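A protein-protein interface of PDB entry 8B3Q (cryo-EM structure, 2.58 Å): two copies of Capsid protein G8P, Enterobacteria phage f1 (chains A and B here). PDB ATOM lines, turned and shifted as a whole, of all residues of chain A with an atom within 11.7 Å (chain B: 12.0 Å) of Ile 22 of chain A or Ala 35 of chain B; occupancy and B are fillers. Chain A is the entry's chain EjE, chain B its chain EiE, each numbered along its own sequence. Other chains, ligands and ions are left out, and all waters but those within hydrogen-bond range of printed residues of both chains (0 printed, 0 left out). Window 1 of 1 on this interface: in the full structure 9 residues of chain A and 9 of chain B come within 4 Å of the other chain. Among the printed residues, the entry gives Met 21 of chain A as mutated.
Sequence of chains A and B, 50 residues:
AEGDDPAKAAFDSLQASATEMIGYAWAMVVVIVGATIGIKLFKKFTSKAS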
ATOM      1  N   ASP A  12       8.237 -25.994  21.279  1.00  0.00           N
ATOM      2  CA  ASP A  12       7.163 -25.087  20.894  1.00  0.00           C
ATOM      3  C   ASP A  12       6.084 -25.822  20.104  1.00  0.00           C
ATOM      4  O   ASP A  12       4.899 -25.688  20.424  1.00  0.00           O
ATOM      5  CB  ASP A  12       7.672 -23.880  20.116  1.00  0.00           C
ATOM      6  CG  ASP A  12       8.597 -22.983  20.917  1.00  0.00           C
ATOM      7  OD1 ASP A  12       8.567 -23.068  22.165  1.00  0.00           O
ATOM      8  OD2 ASP A  12       9.348 -22.211  20.277  1.00  0.00           O
ATOM      9  N   SER A  13       6.511 -26.602  19.101  1.00  0.00           N
ATOM     10  CA  SER A  13       5.582 -27.356  18.276  1.00  0.00           C
ATOM     11  C   SER A  13       4.767 -28.345  19.116  1.00  0.00           C
ATOM     12  O   SER A  13       3.547 -28.392  18.945  1.00  0.00           O
ATOM     13  CB  SER A  13       6.293 -28.043  17.151  1.00  0.00           C
ATOM     14  OG  SER A  13       7.138 -29.063  17.660  1.00  0.00           O
ATOM     15  N   LEU A  14       5.438 -29.127  19.993  1.00  0.00           N
ATOM     16  CA  LEU A  14       4.761 -30.070  20.872  1.00  0.00           C
ATOM     17  C   LEU A  14       3.689 -29.352  21.684  1.00  0.00           C
ATOM     18  O   LEU A  14       2.560 -29.828  21.786  1.00  0.00           O
ATOM     19  CB  LEU A  14       5.754 -30.734  21.819  1.00  0.00           C
ATOM     20  CG  LEU A  14       6.721 -31.716  21.181  1.00  0.00           C
ATOM     21  CD1 LEU A  14       7.939 -31.912  22.059  1.00  0.00           C
ATOM     22  CD2 LEU A  14       6.032 -33.032  21.082  1.00  0.00           C
ATOM     23  N   GLN A  15       4.055 -28.205  22.248  1.00  0.00           N
ATOM     24  CA  GLN A  15       3.130 -27.501  23.109  1.00  0.00           C
ATOM     25  C   GLN A  15       1.932 -26.944  22.344  1.00  0.00           C
ATOM     26  O   GLN A  15       0.845 -26.819  22.919  1.00  0.00           O
ATOM     27  CB  GLN A  15       3.832 -26.402  23.882  1.00  0.00           C
ATOM     28  CG  GLN A  15       2.944 -25.841  24.989  1.00  0.00           C
ATOM     29  CD  GLN A  15       3.631 -24.714  25.697  1.00  0.00           C
ATOM     30  OE1 GLN A  15       4.854 -24.699  25.784  1.00  0.00           O
ATOM     31  NE2 GLN A  15       2.861 -23.732  26.140  1.00  0.00           N
ATOM     32  N   ALA A  16       2.124 -26.628  21.059  1.00  0.00           N
ATOM     33  CA  ALA A  16       1.003 -26.185  20.237  1.00  0.00           C
ATOM     34  C   ALA A  16       0.035 -27.328  19.907  1.00  0.00           C
ATOM     35  O   ALA A  16      -1.177 -27.173  20.075  1.00  0.00           O
ATOM     36  CB  ALA A  16       1.501 -25.523  19.006  1.00  0.00           C
ATOM     37  N   SER A  17       0.565 -28.487  19.498  1.00  0.00           N
ATOM     38  CA  SER A  17      -0.241 -29.683  19.297  1.00  0.00           C
ATOM     39  C   SER A  17      -1.088 -30.027  20.523  1.00  0.00           C
ATOM     40  O   SER A  17      -2.279 -30.325  20.391  1.00  0.00           O
ATOM     41  CB  SER A  17       0.619 -30.826  18.913  1.00  0.00           C
ATOM     42  OG  SER A  17       1.605 -30.374  18.006  1.00  0.00           O
ATOM     43  N   ALA A  18      -0.465 -29.998  21.701  1.00  0.00           N
ATOM     44  CA  ALA A  18      -1.180 -30.296  22.927  1.00  0.00           C
ATOM     45  C   ALA A  18      -2.317 -29.302  23.111  1.00  0.00           C
ATOM     46  O   ALA A  18      -3.445 -29.710  23.380  1.00  0.00           O
ATOM     47  CB  ALA A  18      -0.241 -30.233  24.079  1.00  0.00           C
ATOM     48  N   THR A  19      -2.025 -28.013  22.922  1.00  0.00           N
ATOM     49  CA  THR A  19      -3.069 -27.030  23.108  1.00  0.00           C
ATOM     50  C   THR A  19      -4.276 -27.327  22.216  1.00  0.00           C
ATOM     51  O   THR A  19      -5.409 -27.178  22.677  1.00  0.00           O
ATOM     52  CB  THR A  19      -2.544 -25.614  22.903  1.00  0.00           C
ATOM     53  OG1 THR A  19      -1.728 -25.329  24.034  1.00  0.00           O
ATOM     54  CG2 THR A  19      -3.650 -24.586  22.810  1.00  0.00           C
ATOM     55  N   GLU A  20      -4.044 -27.769  20.970  1.00  0.00           N
ATOM     56  CA  GLU A  20      -5.149 -28.052  20.058  1.00  0.00           C
ATOM     57  C   GLU A  20      -5.974 -29.247  20.535  1.00  0.00           C
ATOM     58  O   GLU A  20      -7.194 -29.120  20.590  1.00  0.00           O
ATOM     59  CB  GLU A  20      -4.674 -28.328  18.642  1.00  0.00           C
ATOM     60  CG  GLU A  20      -4.284 -27.089  17.874  1.00  0.00           C
ATOM     61  CD  GLU A  20      -3.433 -27.376  16.643  1.00  0.00           C
ATOM     62  OE1 GLU A  20      -3.538 -28.495  16.084  1.00  0.00           O
ATOM     63  OE2 GLU A  20      -2.672 -26.477  16.231  1.00  0.00           O
ATOM     64  N   MET A  21      -5.323 -30.376  20.888  1.00  0.00           N
ATOM     65  CA  MET A  21      -6.053 -31.526  21.410  1.00  0.00           C
ATOM     66  C   MET A  21      -6.903 -31.143  22.617  1.00  0.00           C
ATOM     67  O   MET A  21      -8.016 -31.625  22.750  1.00  0.00           O
ATOM     68  CB  MET A  21      -5.180 -32.709  21.827  1.00  0.00           C
ATOM     69  CG  MET A  21      -4.359 -33.197  20.691  1.00  0.00           C
ATOM     70  SD  MET A  21      -4.147 -34.987  20.720  1.00  0.00           S
ATOM     71  CE  MET A  21      -5.865 -35.474  20.889  1.00  0.00           C
ATOM     72  N   ILE A  22      -6.387 -30.309  23.510  1.00  0.00           N
ATOM     73  CA  ILE A  22      -7.175 -29.997  24.678  1.00  0.00           C
ATOM     74  C   ILE A  22      -8.479 -29.355  24.229  1.00  0.00           C
ATOM     75  O   ILE A  22      -9.530 -29.596  24.815  1.00  0.00           O
ATOM     76  CB  ILE A  22      -6.387 -29.071  25.611  1.00  0.00           C
ATOM     77  CG1 ILE A  22      -5.239 -29.850  26.261  1.00  0.00           C
ATOM     78  CG2 ILE A  22      -7.326 -28.406  26.617  1.00  0.00           C
ATOM     79  CD1 ILE A  22      -4.071 -28.991  26.630  1.00  0.00           C
ATOM     80  N   GLY A  23      -8.385 -28.544  23.178  1.00  0.00           N
ATOM     81  CA  GLY A  23      -9.553 -27.904  22.604  1.00  0.00           C
ATOM     82  C   GLY A  23     -10.608 -28.913  22.176  1.00  0.00           C
ATOM     83  O   GLY A  23     -11.774 -28.750  22.526  1.00  0.00           O
ATOM     84  N   TYR A  24     -10.171 -29.955  21.459  1.00  0.00           N
ATOM     85  CA  TYR A  24     -11.089 -30.974  20.977  1.00  0.00           C
ATOM     86  C   TYR A  24     -11.709 -31.731  22.145  1.00  0.00           C
ATOM     87  O   TYR A  24     -12.885 -32.037  22.092  1.00  0.00           O
ATOM     88  CB  TYR A  24     -10.419 -31.980  20.039  1.00  0.00           C
ATOM     89  CG  TYR A  24      -9.651 -31.421  18.873  1.00  0.00           C
ATOM     90  CD1 TYR A  24     -10.160 -30.391  18.081  1.00  0.00           C
ATOM     91  CD2 TYR A  24      -8.388 -31.919  18.579  1.00  0.00           C
ATOM     92  CE1 TYR A  24      -9.397 -29.845  17.057  1.00  0.00           C
ATOM     93  CE2 TYR A  24      -7.638 -31.416  17.525  1.00  0.00           C
ATOM     94  CZ  TYR A  24      -8.134 -30.359  16.780  1.00  0.00           C
ATOM     95  OH  TYR A  24      -7.345 -29.831  15.799  1.00  0.00           O
ATOM     96  N   ALA A  25     -10.924 -32.033  23.180  1.00  0.00           N
ATOM     97  CA  ALA A  25     -11.425 -32.745  24.344  1.00  0.00           C
ATOM     98  C   ALA A  25     -12.541 -31.970  25.042  1.00  0.00           C
ATOM     99  O   ALA A  25     -13.572 -32.557  25.347  1.00  0.00           O
ATOM    100  CB  ALA A  25     -10.296 -33.033  25.283  1.00  0.00           C
ATOM    101  N   TRP A  26     -12.372 -30.656  25.223  1.00  0.00           N
ATOM    102  CA  TRP A  26     -13.423 -29.877  25.866  1.00  0.00           C
ATOM    103  C   TRP A  26     -14.744 -29.953  25.114  1.00  0.00           C
ATOM    104  O   TRP A  26     -15.779 -30.088  25.768  1.00  0.00           O
ATOM    105  CB  TRP A  26     -13.055 -28.412  26.159  1.00  0.00           C
ATOM    106  CG  TRP A  26     -12.351 -28.141  27.462  1.00  0.00           C
ATOM    107  CD1 TRP A  26     -11.004 -27.947  27.656  1.00  0.00           C
ATOM    108  CD2 TRP A  26     -12.951 -28.069  28.774  1.00  0.00           C
ATOM    109  NE1 TRP A  26     -10.730 -27.776  28.987  1.00  0.00           N
ATOM    110  CE2 TRP A  26     -11.902 -27.835  29.699  1.00  0.00           C
ATOM    111  CE3 TRP A  26     -14.264 -28.173  29.266  1.00  0.00           C
ATOM    112  CZ2 TRP A  26     -12.131 -27.714  31.074  1.00  0.00           C
ATOM    113  CZ3 TRP A  26     -14.487 -28.053  30.624  1.00  0.00           C
ATOM    114  CH2 TRP A  26     -13.427 -27.848  31.517  1.00  0.00           C
ATOM    115  N   ALA A  27     -14.690 -29.911  23.772  1.00  0.00           N
ATOM    116  CA  ALA A  27     -15.901 -30.039  22.973  1.00  0.00           C
ATOM    117  C   ALA A  27     -16.665 -31.318  23.300  1.00  0.00           C
ATOM    118  O   ALA A  27     -17.862 -31.270  23.602  1.00  0.00           O
ATOM    119  CB  ALA A  27     -15.553 -30.000  21.530  1.00  0.00           C
ATOM    120  N   MET A  28     -15.936 -32.438  23.323  1.00  0.00           N
ATOM    121  CA  MET A  28     -16.571 -33.715  23.563  1.00  0.00           C
ATOM    122  C   MET A  28     -17.224 -33.793  24.949  1.00  0.00           C
ATOM    123  O   MET A  28     -18.367 -34.232  25.060  1.00  0.00           O
ATOM    124  CB  MET A  28     -15.579 -34.854  23.386  1.00  0.00           C
ATOM    125  CG  MET A  28     -16.321 -36.136  23.255  1.00  0.00           C
ATOM    126  SD  MET A  28     -15.232 -37.520  23.026  1.00  0.00           S
ATOM    127  CE  MET A  28     -15.829 -38.042  21.423  1.00  0.00           C
ATOM    128  N   VAL A  29     -16.510 -33.327  25.972  1.00  0.00           N
ATOM    129  CA  VAL A  29     -16.949 -33.401  27.351  1.00  0.00           C
ATOM    130  C   VAL A  29     -18.268 -32.669  27.487  1.00  0.00           C
ATOM    131  O   VAL A  29     -19.210 -33.223  28.050  1.00  0.00           O
ATOM    132  CB  VAL A  29     -15.907 -32.835  28.330  1.00  0.00           C
ATOM    133  CG1 VAL A  29     -16.402 -32.985  29.734  1.00  0.00           C
ATOM    134  CG2 VAL A  29     -14.656 -33.653  28.254  1.00  0.00           C
ATOM    135  N   VAL A  30     -18.342 -31.483  26.896  1.00  0.00           N
ATOM    136  CA  VAL A  30     -19.555 -30.700  27.012  1.00  0.00           C
ATOM    137  C   VAL A  30     -20.790 -31.414  26.443  1.00  0.00           C
ATOM    138  O   VAL A  30     -21.862 -31.317  27.031  1.00  0.00           O
ATOM    139  CB  VAL A  30     -19.333 -29.318  26.407  1.00  0.00           C
ATOM    140  CG1 VAL A  30     -20.653 -28.629  26.156  1.00  0.00           C
ATOM    141  CG2 VAL A  30     -18.502 -28.517  27.372  1.00  0.00           C
ATOM    142  N   VAL A  31     -20.630 -32.167  25.354  1.00  0.00           N
ATOM    143  CA  VAL A  31     -21.719 -32.948  24.779  1.00  0.00           C
ATOM    144  C   VAL A  31     -22.167 -34.090  25.698  1.00  0.00           C
ATOM    145  O   VAL A  31     -23.347 -34.160  26.055  1.00  0.00           O
ATOM    146  CB  VAL A  31     -21.362 -33.428  23.362  1.00  0.00           C
ATOM    147  CG1 VAL A  31     -22.401 -34.368  22.794  1.00  0.00           C
ATOM    148  CG2 VAL A  31     -21.271 -32.220  22.470  1.00  0.00           C
ATOM    149  N   TRP B  26       8.641 -27.365  32.231  1.00  0.00           N
ATOM    150  CA  TRP B  26       7.675 -26.848  33.189  1.00  0.00           C
ATOM    151  C   TRP B  26       6.489 -26.182  32.507  1.00  0.00           C
ATOM    152  O   TRP B  26       5.364 -26.405  32.954  1.00  0.00           O
ATOM    153  CB  TRP B  26       8.270 -25.921  34.270  1.00  0.00           C
ATOM    154  CG  TRP B  26       8.810 -26.592  35.505  1.00  0.00           C
ATOM    155  CD1 TRP B  26      10.123 -26.870  35.792  1.00  0.00           C
ATOM    156  CD2 TRP B  26       8.048 -27.132  36.609  1.00  0.00           C
ATOM    157  NE1 TRP B  26      10.228 -27.543  36.979  1.00  0.00           N
ATOM    158  CE2 TRP B  26       8.974 -27.718  37.507  1.00  0.00           C
ATOM    159  CE3 TRP B  26       6.684 -27.170  36.942  1.00  0.00           C
ATOM    160  CZ2 TRP B  26       8.577 -28.326  38.701  1.00  0.00           C
ATOM    161  CZ3 TRP B  26       6.294 -27.778  38.119  1.00  0.00           C
ATOM    162  CH2 TRP B  26       7.230 -28.362  38.978  1.00  0.00           C
ATOM    163  N   ALA B  27       6.742 -25.426  31.424  1.00  0.00           N
ATOM    164  CA  ALA B  27       5.659 -24.792  30.683  1.00  0.00           C
ATOM    165  C   ALA B  27       4.635 -25.806  30.188  1.00  0.00           C
ATOM    166  O   ALA B  27       3.441 -25.656  30.457  1.00  0.00           O
ATOM    167  CB  ALA B  27       6.207 -24.024  29.546  1.00  0.00           C
ATOM    168  N   MET B  28       5.139 -26.890  29.594  1.00  0.00           N
ATOM    169  CA  MET B  28       4.249 -27.895  29.052  1.00  0.00           C
ATOM    170  C   MET B  28       3.391 -28.558  30.135  1.00  0.00           C
ATOM    171  O   MET B  28       2.185 -28.702  29.959  1.00  0.00           O
ATOM    172  CB  MET B  28       5.020 -28.965  28.294  1.00  0.00           C
ATOM    173  CG  MET B  28       4.091 -29.687  27.392  1.00  0.00           C
ATOM    174  SD  MET B  28       4.948 -30.923  26.451  1.00  0.00           S
ATOM    175  CE  MET B  28       4.384 -30.379  24.842  1.00  0.00           C
ATOM    176  N   VAL B  29       4.020 -28.935  31.243  1.00  0.00           N
ATOM    177  CA  VAL B  29       3.373 -29.654  32.321  1.00  0.00           C
ATOM    178  C   VAL B  29       2.216 -28.824  32.839  1.00  0.00           C
ATOM    179  O   VAL B  29       1.114 -29.349  32.984  1.00  0.00           O
ATOM    180  CB  VAL B  29       4.342 -30.004  33.464  1.00  0.00           C
ATOM    181  CG1 VAL B  29       3.625 -30.806  34.498  1.00  0.00           C
ATOM    182  CG2 VAL B  29       5.415 -30.905  32.950  1.00  0.00           C
ATOM    183  N   VAL B  30       2.456 -27.533  33.030  1.00  0.00           N
ATOM    184  CA  VAL B  30       1.407 -26.688  33.558  1.00  0.00           C
ATOM    185  C   VAL B  30       0.155 -26.647  32.672  1.00  0.00           C
ATOM    186  O   VAL B  30      -0.954 -26.645  33.199  1.00  0.00           O
ATOM    187  CB  VAL B  30       1.965 -25.302  33.872  1.00  0.00           C
ATOM    188  CG1 VAL B  30       0.842 -24.321  34.068  1.00  0.00           C
ATOM    189  CG2 VAL B  30       2.772 -25.399  35.136  1.00  0.00           C
ATOM    190  N   VAL B  31       0.327 -26.676  31.350  1.00  0.00           N
ATOM    191  CA  VAL B  31      -0.787 -26.732  30.410  1.00  0.00           C
ATOM    192  C   VAL B  31      -1.569 -28.048  30.509  1.00  0.00           C
ATOM    193  O   VAL B  31      -2.776 -28.024  30.735  1.00  0.00           O
ATOM    194  CB  VAL B  31      -0.304 -26.415  28.983  1.00  0.00           C
ATOM    195  CG1 VAL B  31      -1.345 -26.679  27.923  1.00  0.00           C
ATOM    196  CG2 VAL B  31       0.084 -24.966  28.944  1.00  0.00           C
ATOM    197  N   ILE B  32      -0.883 -29.178  30.341  1.00  0.00           N
ATOM    198  CA  ILE B  32      -1.516 -30.477  30.381  1.00  0.00           C
ATOM    199  C   ILE B  32      -2.226 -30.671  31.718  1.00  0.00           C
ATOM    200  O   ILE B  32      -3.410 -30.992  31.711  1.00  0.00           O
ATOM    201  CB  ILE B  32      -0.473 -31.566  30.089  1.00  0.00           C
ATOM    202  CG1 ILE B  32      -0.102 -31.583  28.610  1.00  0.00           C
ATOM    203  CG2 ILE B  32      -0.985 -32.907  30.513  1.00  0.00           C
ATOM    204  CD1 ILE B  32       1.299 -32.040  28.395  1.00  0.00           C
ATOM    205  N   VAL B  33      -1.542 -30.424  32.846  1.00  0.00           N
ATOM    206  CA  VAL B  33      -2.174 -30.654  34.138  1.00  0.00           C
ATOM    207  C   VAL B  33      -3.366 -29.726  34.346  1.00  0.00           C
ATOM    208  O   VAL B  33      -4.402 -30.162  34.843  1.00  0.00           O
ATOM    209  CB  VAL B  33      -1.208 -30.553  35.326  1.00  0.00           C
ATOM    210  CG1 VAL B  33      -1.980 -30.415  36.630  1.00  0.00           C
ATOM    211  CG2 VAL B  33      -0.263 -31.741  35.372  1.00  0.00           C
ATOM    212  N   GLY B  34      -3.223 -28.460  33.955  1.00  0.00           N
ATOM    213  CA  GLY B  34      -4.348 -27.533  33.958  1.00  0.00           C
ATOM    214  C   GLY B  34      -5.625 -28.130  33.369  1.00  0.00           C
ATOM    215  O   GLY B  34      -6.701 -27.974  33.941  1.00  0.00           O
ATOM    216  N   ALA B  35      -5.502 -28.824  32.237  1.00  0.00           N
ATOM    217  CA  ALA B  35      -6.677 -29.347  31.563  1.00  0.00           C
ATOM    218  C   ALA B  35      -7.215 -30.597  32.253  1.00  0.00           C
ATOM    219  O   ALA B  35      -8.419 -30.720  32.436  1.00  0.00           O
ATOM    220  CB  ALA B  35      -6.320 -29.655  30.153  1.00  0.00           C
ATOM    221  N   THR B  36      -6.329 -31.523  32.616  1.00  0.00           N
ATOM    222  CA  THR B  36      -6.743 -32.703  33.360  1.00  0.00           C
ATOM    223  C   THR B  36      -7.575 -32.331  34.591  1.00  0.00           C
ATOM    224  O   THR B  36      -8.681 -32.837  34.724  1.00  0.00           O
ATOM    225  CB  THR B  36      -5.519 -33.541  33.718  1.00  0.00           C
ATOM    226  OG1 THR B  36      -5.124 -34.064  32.453  1.00  0.00           O
ATOM    227  CG2 THR B  36      -5.800 -34.647  34.707  1.00  0.00           C
ATOM    228  N   ILE B  37      -7.082 -31.415  35.429  1.00  0.00           N
ATOM    229  CA  ILE B  37      -7.765 -31.054  36.655  1.00  0.00           C
ATOM    230  C   ILE B  37      -9.040 -30.295  36.319  1.00  0.00           C
ATOM    231  O   ILE B  37     -10.060 -30.487  36.978  1.00  0.00           O
ATOM    232  CB  ILE B  37      -6.840 -30.227  37.574  1.00  0.00           C
ATOM    233  CG1 ILE B  37      -5.653 -31.036  38.083  1.00  0.00           C
ATOM    234  CG2 ILE B  37      -7.598 -29.639  38.743  1.00  0.00           C
ATOM    235  CD1 ILE B  37      -5.995 -32.437  38.522  1.00  0.00           C
ATOM    236  N   GLY B  38      -8.970 -29.435  35.297  1.00  0.00           N
ATOM    237  CA  GLY B  38     -10.151 -28.709  34.857  1.00  0.00           C
ATOM    238  C   GLY B  38     -11.329 -29.633  34.549  1.00  0.00           C
ATOM    239  O   GLY B  38     -12.394 -29.462  35.136  1.00  0.00           O
ATOM    240  N   ILE B  39     -11.087 -30.671  33.741  1.00  0.00           N
ATOM    241  CA  ILE B  39     -12.166 -31.554  33.342  1.00  0.00           C
ATOM    242  C   ILE B  39     -12.692 -32.314  34.554  1.00  0.00           C
ATOM    243  O   ILE B  39     -13.902 -32.419  34.721  1.00  0.00           O
ATOM    244  CB  ILE B  39     -11.705 -32.458  32.204  1.00  0.00           C
ATOM    245  CG1 ILE B  39     -11.514 -31.614  30.953  1.00  0.00           C
ATOM    246  CG2 ILE B  39     -12.673 -33.580  31.924  1.00  0.00           C
ATOM    247  CD1 ILE B  39     -10.764 -32.335  29.885  1.00  0.00           C
ATOM    248  N   LYS B  40     -11.785 -32.795  35.402  1.00  0.00           N
ATOM    249  CA  LYS B  40     -12.174 -33.507  36.607  1.00  0.00           C
ATOM    250  C   LYS B  40     -13.128 -32.671  37.465  1.00  0.00           C
ATOM    251  O   LYS B  40     -14.172 -33.184  37.843  1.00  0.00           O
ATOM    252  CB  LYS B  40     -10.916 -33.878  37.381  1.00  0.00           C
ATOM    253  CG  LYS B  40     -11.086 -34.732  38.620  1.00  0.00           C
ATOM    254  CD  LYS B  40      -9.764 -34.878  39.362  1.00  0.00           C
ATOM    255  CE  LYS B  40      -9.831 -35.723  40.617  1.00  0.00           C
ATOM    256  NZ  LYS B  40      -8.913 -35.224  41.666  1.00  0.00           N
ATOM    257  N   LEU B  41     -12.814 -31.395  37.718  1.00  0.00           N
ATOM    258  CA  LEU B  41     -13.700 -30.594  38.546  1.00  0.00           C
ATOM    259  C   LEU B  41     -15.036 -30.297  37.883  1.00  0.00           C
ATOM    260  O   LEU B  41     -16.061 -30.265  38.571  1.00  0.00           O
ATOM    261  CB  LEU B  41     -12.993 -29.335  39.025  1.00  0.00           C
ATOM    262  CG  LEU B  41     -11.846 -29.648  39.981  1.00  0.00           C
ATOM    263  CD1 LEU B  41     -11.096 -28.397  40.353  1.00  0.00           C
ATOM    264  CD2 LEU B  41     -12.345 -30.330  41.246  1.00  0.00           C
ATOM    265  N   PHE B  42     -15.018 -30.113  36.559  1.00  0.00           N
ATOM    266  CA  PHE B  42     -16.247 -29.836  35.838  1.00  0.00           C
ATOM    267  C   PHE B  42     -17.211 -31.005  35.987  1.00  0.00           C
ATOM    268  O   PHE B  42     -18.372 -30.806  36.314  1.00  0.00           O
ATOM    269  CB  PHE B  42     -15.910 -29.626  34.371  1.00  0.00           C
ATOM    270  CG  PHE B  42     -17.124 -29.403  33.521  1.00  0.00           C
ATOM    271  CD1 PHE B  42     -17.904 -28.261  33.674  1.00  0.00           C
ATOM    272  CD2 PHE B  42     -17.493 -30.350  32.571  1.00  0.00           C
ATOM    273  CE1 PHE B  42     -19.030 -28.064  32.879  1.00  0.00           C
ATOM    274  CE2 PHE B  42     -18.614 -30.150  31.773  1.00  0.00           C
ATOM    275  CZ  PHE B  42     -19.391 -29.011  31.940  1.00  0.00           C
ATOM    276  N   LYS B  43     -16.689 -32.229  35.810  1.00  0.00           N
ATOM    277  CA  LYS B  43     -17.506 -33.426  35.974  1.00  0.00           C
ATOM    278  C   LYS B  43     -18.077 -33.527  37.389  1.00  0.00           C
ATOM    279  O   LYS B  43     -19.256 -33.825  37.533  1.00  0.00           O
ATOM    280  CB  LYS B  43     -16.811 -34.728  35.553  1.00  0.00           C
ATOM    281  CG  LYS B  43     -16.362 -34.812  34.102  1.00  0.00           C
ATOM    282  CD  LYS B  43     -16.326 -36.208  33.545  1.00  0.00           C
ATOM    283  CE  LYS B  43     -14.928 -36.773  33.407  1.00  0.00           C
ATOM    284  NZ  LYS B  43     -14.940 -38.076  32.700  1.00  0.00           N
ATOM    285  N   LYS B  44     -17.261 -33.215  38.400  1.00  0.00           N
ATOM    286  CA  LYS B  44     -17.616 -33.390  39.798  1.00  0.00           C
ATOM    287  C   LYS B  44     -18.660 -32.365  40.241  1.00  0.00           C
ATOM    288  O   LYS B  44     -19.712 -32.730  40.768  1.00  0.00           O
ATOM    289  CB  LYS B  44     -16.369 -33.272  40.679  1.00  0.00           C
ATOM    290  CG  LYS B  44     -16.694 -33.378  42.160  1.00  0.00           C
ATOM    291  CD  LYS B  44     -15.806 -32.593  43.086  1.00  0.00           C
ATOM    292  CE  LYS B  44     -14.447 -33.197  43.396  1.00  0.00           C
ATOM    293  NZ  LYS B  44     -14.520 -34.644  43.701  1.00  0.00           N
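The backbone carbonyl oxygen (O) of Gln 15 of chain A sits at hydrogen-bond distance from the side-chain hydroxyl (OG1) of Thr 19 of chain A.
Among the printed residues, merely in contact across the chains: Leu 14 of chain A with Met 28 of chain B (3.3 Å), Gln 15 of chain A with Met 28 of chain B (3.4 Å), Ile 22 of chain A with Val 31 of chain B (3.8 Å), Ile 22 of chain A with Ala 35 of chain B (3.9 Å) and Trp 26 of chain A with Ile 39 of chain B (3.95 Å).
Of chain B, only Val 31 and Ala 35 come within 4 Å of Ile 22 of chain A.
Ala 35 of chain B touches just one residue of chain A: Ile 22 (3.9 Å).
No residue of chain B comes within 4 Å of Ala 18 of chain A.
No residue of chain B comes within 4 Å of Met 21 of chain A.
No residue of chain B comes within 4 Å of Gly 23 of chain A.
Tyr 24 of chain A touches none of the printed residues of chain B.
Of chain B, only Ile 39 comes within 4 Å of Trp 26 of chain A.
No residue of chain A comes within 4 Å of Ile 32 of chain B.
No residue of chain A comes within 4 Å of Val 33 of chain B.
No residue of chain A comes within 4 Å of Gly 34 of chain B.
No residue of chain A comes within 4 Å of Ile 37 of chain B.
Gly 38 of chain B touches none of the printed residues of chain A.
Printed residues of chain A within 4 Å of Ile 39 of chain B: Trp 26.
Printed residues of chain B within 4 Å of Leu 14 of chain A: Met 28 (3.3 Å).
Of the printed residues of chain B, Gln 15 of chain A touches Met 28.
Printed residues of chain A within 4 Å of Met 28 of chain B: Leu 14 (3.3 Å) and Gln 15 (3.4 Å).
Leu 41 of chain B touches none of the printed residues of chain A.
The nearest residue of chain B that does not touch Ile 22 of chain A is Ile 32 of chain B (4.8 Å).
The nearest printed residue of chain B that does not touch Leu 14 of chain A is Ile 32 of chain B (7.1 Å).
Printed residues of chain A that touch a printed residue of chain B: Leu 14, Gln 15, Ile 22 and Trp 26.
Hydrophobic or aromatic side chains of chain A that line the printed part of chain B: Leu 14, Ile 22 and Trp 26.
Along chain A the printed residues that touch a printed residue of chain B span positions 14 to 26.
Of the 19 printed residues of chain B, 4 touch a printed residue of chain A.
Hydrophobic or aromatic side chains of chain B that line the printed part of chain A: Met 28, Val 31, Ala 35 and Ile 39.
Among the printed residues, no Asp or Glu carboxylate lies within 4 Å of a Lys or Arg side-chain nitrogen of the other chain.
Positions printed for both chains: 26, 27, 28, 29, 30 and 31.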
